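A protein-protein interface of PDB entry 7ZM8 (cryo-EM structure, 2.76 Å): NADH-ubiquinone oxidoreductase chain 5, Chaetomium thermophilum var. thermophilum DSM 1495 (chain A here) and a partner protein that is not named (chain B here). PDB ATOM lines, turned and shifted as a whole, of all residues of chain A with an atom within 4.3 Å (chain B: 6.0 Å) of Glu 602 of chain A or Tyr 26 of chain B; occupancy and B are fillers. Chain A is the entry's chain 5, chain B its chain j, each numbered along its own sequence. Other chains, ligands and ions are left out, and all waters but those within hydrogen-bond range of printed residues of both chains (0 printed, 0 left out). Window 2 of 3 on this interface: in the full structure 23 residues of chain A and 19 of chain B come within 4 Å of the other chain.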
ATOM      1  N   ASP A 597      -3.902  -6.474  12.049  1.00  0.00           N
ATOM      2  CA  ASP A 597      -5.121  -5.906  12.690  1.00  0.00           C
ATOM      3  C   ASP A 597      -5.392  -4.493  12.204  1.00  0.00           C
ATOM      4  O   ASP A 597      -6.555  -4.189  11.911  1.00  0.00           O
ATOM      5  CB  ASP A 597      -4.907  -5.712  14.187  1.00  0.00           C
ATOM      6  CG  ASP A 597      -5.006  -6.982  15.004  1.00  0.00           C
ATOM      7  OD1 ASP A 597      -5.895  -7.797  14.709  1.00  0.00           O
ATOM      8  OD2 ASP A 597      -4.200  -7.135  15.935  1.00  0.00           O
ATOM      9  N   LYS A 598      -4.347  -3.673  12.135  1.00  0.00           N
ATOM     10  CA  LYS A 598      -4.493  -2.254  11.734  1.00  0.00           C
ATOM     11  C   LYS A 598      -4.063  -2.157  10.277  1.00  0.00           C
ATOM     12  O   LYS A 598      -4.008  -1.051   9.751  1.00  0.00           O
ATOM     13  CB  LYS A 598      -3.624  -1.364  12.626  1.00  0.00           C
ATOM     14  CG  LYS A 598      -4.232  -0.930  13.953  1.00  0.00           C
ATOM     15  CD  LYS A 598      -4.530  -2.045  14.928  1.00  0.00           C
ATOM     16  CE  LYS A 598      -5.015  -1.534  16.267  1.00  0.00           C
ATOM     17  NZ  LYS A 598      -6.129  -0.570  16.112  1.00  0.00           N
ATOM     18  N   GLY A 599      -3.757  -3.291   9.661  1.00  0.00           N
ATOM     19  CA  GLY A 599      -3.313  -3.265   8.288  1.00  0.00           C
ATOM     20  C   GLY A 599      -4.258  -3.914   7.305  1.00  0.00           C
ATOM     21  O   GLY A 599      -5.251  -3.320   6.882  1.00  0.00           O
ATOM     22  N   SER A 600      -3.934  -5.152   6.938  1.00  0.00           N
ATOM     23  CA  SER A 600      -4.633  -5.835   5.861  1.00  0.00           C
ATOM     24  C   SER A 600      -6.032  -6.281   6.264  1.00  0.00           C
ATOM     25  O   SER A 600      -6.893  -6.455   5.399  1.00  0.00           O
ATOM     26  CB  SER A 600      -3.802  -7.027   5.402  1.00  0.00           C
ATOM     27  OG  SER A 600      -3.266  -7.716   6.513  1.00  0.00           O
ATOM     28  N   ILE A 601      -6.293  -6.362   7.555  1.00  0.00           N
ATOM     29  CA  ILE A 601      -7.619  -6.871   7.967  1.00  0.00           C
ATOM     30  C   ILE A 601      -8.597  -5.711   7.760  1.00  0.00           C
ATOM     31  O   ILE A 601      -9.762  -5.966   7.422  1.00  0.00           O
ATOM     32  CB  ILE A 601      -7.576  -7.426   9.407  1.00  0.00           C
ATOM     33  CG1 ILE A 601      -6.771  -8.725   9.497  1.00  0.00           C
ATOM     34  CG2 ILE A 601      -8.969  -7.594   9.991  1.00  0.00           C
ATOM     35  CD1 ILE A 601      -7.199  -9.781   8.515  1.00  0.00           C
ATOM     36  N   GLU A 602      -8.114  -4.474   7.903  1.00  0.00           N
ATOM     37  CA  GLU A 602      -8.993  -3.341   7.648  1.00  0.00           C
ATOM     38  C   GLU A 602      -8.988  -2.944   6.178  1.00  0.00           C
ATOM     39  O   GLU A 602     -10.000  -2.463   5.662  1.00  0.00           O
ATOM     40  CB  GLU A 602      -8.611  -2.156   8.532  1.00  0.00           C
ATOM     41  CG  GLU A 602      -8.668  -2.462  10.007  1.00  0.00           C
ATOM     42  CD  GLU A 602      -8.987  -1.241  10.839  1.00  0.00           C
ATOM     43  OE1 GLU A 602      -9.580  -0.292  10.286  1.00  0.00           O
ATOM     44  OE2 GLU A 602      -8.646  -1.223  12.041  1.00  0.00           O
ATOM     45  N   LEU A 603      -7.891  -3.204   5.469  1.00  0.00           N
ATOM     46  CA  LEU A 603      -7.824  -2.949   4.002  1.00  0.00           C
ATOM     47  C   LEU A 603      -8.644  -4.000   3.255  1.00  0.00           C
ATOM     48  O   LEU A 603      -9.472  -3.609   2.421  1.00  0.00           O
ATOM     49  CB  LEU A 603      -6.396  -2.886   3.470  1.00  0.00           C
ATOM     50  CG  LEU A 603      -6.290  -2.256   2.080  1.00  0.00           C
ATOM     51  CD1 LEU A 603      -7.102  -0.971   2.001  1.00  0.00           C
ATOM     52  CD2 LEU A 603      -4.848  -1.985   1.694  1.00  0.00           C
ATOM     53  N   PHE A 604      -8.412  -5.285   3.512  1.00  0.00           N
ATOM     54  CA  PHE A 604      -9.305  -6.303   2.901  1.00  0.00           C
ATOM     55  C   PHE A 604     -10.471  -6.472   3.861  1.00  0.00           C
ATOM     56  O   PHE A 604     -10.681  -7.578   4.375  1.00  0.00           O
ATOM     57  CB  PHE A 604      -8.579  -7.619   2.607  1.00  0.00           C
ATOM     58  CG  PHE A 604      -9.334  -8.609   1.759  1.00  0.00           C
ATOM     59  CD1 PHE A 604      -9.617  -8.336   0.434  1.00  0.00           C
ATOM     60  CD2 PHE A 604      -9.731  -9.828   2.281  1.00  0.00           C
ATOM     61  CE1 PHE A 604     -10.301  -9.253  -0.347  1.00  0.00           C
ATOM     62  CE2 PHE A 604     -10.416 -10.744   1.500  1.00  0.00           C
ATOM     63  CZ  PHE A 604     -10.698 -10.455   0.187  1.00  0.00           C
ATOM     64  N   GLY A 605     -11.141  -5.367   4.164  1.00  0.00           N
ATOM     65  CA  GLY A 605     -12.325  -5.453   5.023  1.00  0.00           C
ATOM     66  C   GLY A 605     -13.089  -4.157   5.091  1.00  0.00           C
ATOM     67  O   GLY A 605     -13.203  -3.539   4.051  1.00  0.00           O
ATOM     68  N   PRO A 606     -13.498  -3.647   6.283  1.00  0.00           N
ATOM     69  CA  PRO A 606     -14.393  -2.480   6.357  1.00  0.00           C
ATOM     70  C   PRO A 606     -13.827  -1.222   5.727  1.00  0.00           C
ATOM     71  O   PRO A 606     -14.555  -0.498   5.043  1.00  0.00           O
ATOM     72  CB  PRO A 606     -14.602  -2.299   7.867  1.00  0.00           C
ATOM     73  CG  PRO A 606     -14.135  -3.548   8.490  1.00  0.00           C
ATOM     74  CD  PRO A 606     -13.074  -4.097   7.616  1.00  0.00           C
ATOM     75  N   TYR A 607     -12.540  -0.944   5.923  1.00  0.00           N
ATOM     76  CA  TYR A 607     -11.979   0.303   5.420  1.00  0.00           C
ATOM     77  C   TYR A 607     -11.793   0.261   3.909  1.00  0.00           C
ATOM     78  O   TYR A 607     -12.036   1.256   3.222  1.00  0.00           O
ATOM     79  CB  TYR A 607     -10.661   0.601   6.126  1.00  0.00           C
ATOM     80  CG  TYR A 607     -10.019   1.890   5.694  1.00  0.00           C
ATOM     81  CD1 TYR A 607     -10.652   3.105   5.896  1.00  0.00           C
ATOM     82  CD2 TYR A 607      -8.784   1.892   5.079  1.00  0.00           C
ATOM     83  CE1 TYR A 607     -10.063   4.280   5.503  1.00  0.00           C
ATOM     84  CE2 TYR A 607      -8.193   3.055   4.684  1.00  0.00           C
ATOM     85  CZ  TYR A 607      -8.831   4.248   4.896  1.00  0.00           C
ATOM     86  OH  TYR A 607      -8.232   5.416   4.490  1.00  0.00           O
ATOM     87  N   GLY A 608     -11.468  -0.895   3.356  1.00  0.00           N
ATOM     88  CA  GLY A 608     -11.304  -1.037   1.902  1.00  0.00           C
ATOM     89  C   GLY A 608     -12.634  -1.137   1.191  1.00  0.00           C
ATOM     90  O   GLY A 608     -12.700  -0.758   0.021  1.00  0.00           O
ATOM     91  N   MET B  21      -1.184   8.770  16.317  1.00  0.00           N
ATOM     92  CA  MET B  21      -0.636   8.026  15.190  1.00  0.00           C
ATOM     93  C   MET B  21      -1.123   6.586  15.196  1.00  0.00           C
ATOM     94  O   MET B  21      -1.483   6.040  14.149  1.00  0.00           O
ATOM     95  CB  MET B  21       0.891   8.082  15.224  1.00  0.00           C
ATOM     96  CG  MET B  21       1.584   7.516  13.989  1.00  0.00           C
ATOM     97  SD  MET B  21       1.817   5.725  14.018  1.00  0.00           S
ATOM     98  CE  MET B  21       3.118   5.572  15.231  1.00  0.00           C
ATOM     99  N   ILE B  22      -1.111   5.940  16.353  1.00  0.00           N
ATOM    100  CA  ILE B  22      -1.510   4.507  16.427  1.00  0.00           C
ATOM    101  C   ILE B  22      -2.982   4.394  16.003  1.00  0.00           C
ATOM    102  O   ILE B  22      -3.300   3.490  15.219  1.00  0.00           O
ATOM    103  CB  ILE B  22      -1.191   3.973  17.835  1.00  0.00           C
ATOM    104  CG1 ILE B  22       0.320   3.839  18.024  1.00  0.00           C
ATOM    105  CG2 ILE B  22      -1.903   2.660  18.102  1.00  0.00           C
ATOM    106  CD1 ILE B  22       0.750   3.513  19.432  1.00  0.00           C
ATOM    107  N   SER B  23      -3.829   5.325  16.433  1.00  0.00           N
ATOM    108  CA  SER B  23      -5.282   5.310  16.126  1.00  0.00           C
ATOM    109  C   SER B  23      -5.599   5.485  14.640  1.00  0.00           C
ATOM    110  O   SER B  23      -6.539   4.823  14.178  1.00  0.00           O
ATOM    111  CB  SER B  23      -5.998   6.347  16.933  1.00  0.00           C
ATOM    112  OG  SER B  23      -5.866   6.076  18.319  1.00  0.00           O
ATOM    113  N   ASN B  24      -4.874   6.318  13.910  1.00  0.00           N
ATOM    114  CA  ASN B  24      -5.250   6.596  12.505  1.00  0.00           C
ATOM    115  C   ASN B  24      -4.389   5.777  11.550  1.00  0.00           C
ATOM    116  O   ASN B  24      -4.650   5.843  10.360  1.00  0.00           O
ATOM    117  CB  ASN B  24      -5.129   8.093  12.244  1.00  0.00           C
ATOM    118  CG  ASN B  24      -6.119   8.911  13.042  1.00  0.00           C
ATOM    119  OD1 ASN B  24      -7.313   8.883  12.766  1.00  0.00           O
ATOM    120  ND2 ASN B  24      -5.632   9.653  14.021  1.00  0.00           N
ATOM    121  N   ARG B  25      -3.454   4.975  12.052  1.00  0.00           N
ATOM    122  CA  ARG B  25      -2.460   4.206  11.244  1.00  0.00           C
ATOM    123  C   ARG B  25      -3.051   3.429  10.060  1.00  0.00           C
ATOM    124  O   ARG B  25      -2.376   3.371   9.027  1.00  0.00           O
ATOM    125  CB  ARG B  25      -1.691   3.292  12.204  1.00  0.00           C
ATOM    126  CG  ARG B  25      -0.509   2.575  11.579  1.00  0.00           C
ATOM    127  CD  ARG B  25       0.080   1.494  12.460  1.00  0.00           C
ATOM    128  NE  ARG B  25       1.043   0.752  11.667  1.00  0.00           N
ATOM    129  CZ  ARG B  25       2.342   1.009  11.618  1.00  0.00           C
ATOM    130  NH1 ARG B  25       3.128   0.277  10.851  1.00  0.00           N
ATOM    131  NH2 ARG B  25       2.856   1.978  12.353  1.00  0.00           N
ATOM    132  N   TYR B  26      -4.229   2.836  10.211  1.00  0.00           N
ATOM    133  CA  TYR B  26      -4.836   1.985   9.153  1.00  0.00           C
ATOM    134  C   TYR B  26      -5.049   2.797   7.874  1.00  0.00           C
ATOM    135  O   TYR B  26      -4.939   2.244   6.783  1.00  0.00           O
ATOM    136  CB  TYR B  26      -6.144   1.375   9.678  1.00  0.00           C
ATOM    137  CG  TYR B  26      -7.264   2.362   9.879  1.00  0.00           C
ATOM    138  CD1 TYR B  26      -7.309   3.172  11.000  1.00  0.00           C
ATOM    139  CD2 TYR B  26      -8.270   2.503   8.937  1.00  0.00           C
ATOM    140  CE1 TYR B  26      -8.323   4.094  11.185  1.00  0.00           C
ATOM    141  CE2 TYR B  26      -9.291   3.421   9.107  1.00  0.00           C
ATOM    142  CZ  TYR B  26      -9.316   4.222  10.233  1.00  0.00           C
ATOM    143  OH  TYR B  26     -10.318   5.129  10.412  1.00  0.00           O
ATOM    144  N   LYS B  27      -5.400   4.061   8.011  1.00  0.00           N
ATOM    145  CA  LYS B  27      -5.621   4.940   6.852  1.00  0.00           C
ATOM    146  C   LYS B  27      -4.368   4.965   5.974  1.00  0.00           C
ATOM    147  O   LYS B  27      -4.471   5.487   4.853  1.00  0.00           O
ATOM    148  CB  LYS B  27      -5.966   6.327   7.384  1.00  0.00           C
ATOM    149  CG  LYS B  27      -7.355   6.485   7.978  1.00  0.00           C
ATOM    150  CD  LYS B  27      -7.454   7.666   8.908  1.00  0.00           C
ATOM    151  CE  LYS B  27      -6.679   8.867   8.415  1.00  0.00           C
ATOM    152  NZ  LYS B  27      -6.778  10.006   9.359  1.00  0.00           N
ATOM    153  N   TYR B  28      -3.238   4.403   6.433  1.00  0.00           N
ATOM    154  CA  TYR B  28      -2.078   4.497   5.559  1.00  0.00           C
ATOM    155  C   TYR B  28      -1.493   3.145   5.182  1.00  0.00           C
ATOM    156  O   TYR B  28      -0.394   3.097   4.626  1.00  0.00           O
ATOM    157  CB  TYR B  28      -0.994   5.372   6.189  1.00  0.00           C
ATOM    158  CG  TYR B  28      -1.492   6.691   6.721  1.00  0.00           C
ATOM    159  CD1 TYR B  28      -2.166   6.773   7.929  1.00  0.00           C
ATOM    160  CD2 TYR B  28      -1.341   7.851   5.980  1.00  0.00           C
ATOM    161  CE1 TYR B  28      -2.630   7.969   8.400  1.00  0.00           C
ATOM    162  CE2 TYR B  28      -1.806   9.049   6.444  1.00  0.00           C
ATOM    163  CZ  TYR B  28      -2.449   9.105   7.651  1.00  0.00           C
ATOM    164  OH  TYR B  28      -2.914  10.312   8.112  1.00  0.00           O
ATOM    165  N   PHE B  29      -2.195   2.051   5.442  1.00  0.00           N
ATOM    166  CA  PHE B  29      -1.702   0.746   5.028  1.00  0.00           C
ATOM    167  C   PHE B  29      -1.790   0.599   3.515  1.00  0.00           C
ATOM    168  O   PHE B  29      -2.807   0.925   2.898  1.00  0.00           O
ATOM    169  CB  PHE B  29      -2.495  -0.368   5.716  1.00  0.00           C
ATOM    170  CG  PHE B  29      -2.093  -1.754   5.291  1.00  0.00           C
ATOM    171  CD1 PHE B  29      -1.060  -2.414   5.917  1.00  0.00           C
ATOM    172  CD2 PHE B  29      -2.760  -2.395   4.270  1.00  0.00           C
ATOM    173  CE1 PHE B  29      -0.692  -3.668   5.532  1.00  0.00           C
ATOM    174  CE2 PHE B  29      -2.392  -3.652   3.876  1.00  0.00           C
ATOM    175  CZ  PHE B  29      -1.358  -4.293   4.512  1.00  0.00           C
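The backbone carbonyl oxygen (O) of Glu 602 of chain A sits at hydrogen-bond distance from the backbone NH (N) of Gly 608 of chain A (3.2 Å).
The backbone carbonyl oxygen (O) of Leu 603 of chain A lies close to the backbone NH (N) of Gly 608 of chain A (3.5 Å).
The backbone carbonyl oxygen (O) of Glu 602 of chain A sits at hydrogen-bond distance from the backbone NH (N) of Tyr 607 of chain A, at 3.0 Å.
Among the printed residues, merely in contact across the chains: Lys 598 of chain A with Tyr 26 of chain B (3.2 Å), Leu 603 of chain A with Phe 29 of chain B (3.3 Å), Glu 602 of chain A with Tyr 26 of chain B (3.4 Å), Gly 599 of chain A with Phe 29 of chain B (3.4 Å), Tyr 607 of chain A with Tyr 26 of chain B (3.5 Å), Tyr 607 of chain A with Lys 27 of chain B (3.6 Å) and Ser 600 of chain A with Phe 29 of chain B (3.6 Å).
Of chain B, only Tyr 26 comes within 4 Å of Glu 602 of chain A.
Of chain A, only Lys 598 (3.2 Å), Glu 602 (3.4 Å) and Tyr 607 (3.5 Å) come within 4 Å of Tyr 26 of chain B.
Of the printed residues of chain A, Phe 29 of chain B touches Gly 599 (3.4 Å), Ser 600 (3.6 Å) and Leu 603 (3.3 Å).
Printed residues of chain B within 4 Å of Gly 599 of chain A: Phe 29.
Printed residues of chain B within 4 Å of Leu 603 of chain A: Phe 29 (3.3 Å).
Printed residues of chain B within 4 Å of Ser 600 of chain A: Phe 29.
Printed residues of chain B within 4 Å of Lys 598 of chain A: Tyr 26 (3.2 Å).
The nearest printed residue of chain B that does not touch Glu 602 of chain A is Lys 27 of chain B (6.4 Å).
The nearest printed residue of chain A that does not touch Tyr 26 of chain B is Gly 599 of chain A (5.2 Å).
The nearest printed residue of chain A that does not touch Lys 27 of chain B is Lys 598 of chain A (5.6 Å).
Of the 12 printed residues of chain A, 6 touch a printed residue of chain B.
Along chain A the printed residues that touch a printed residue of chain B span positions 598 to 607.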
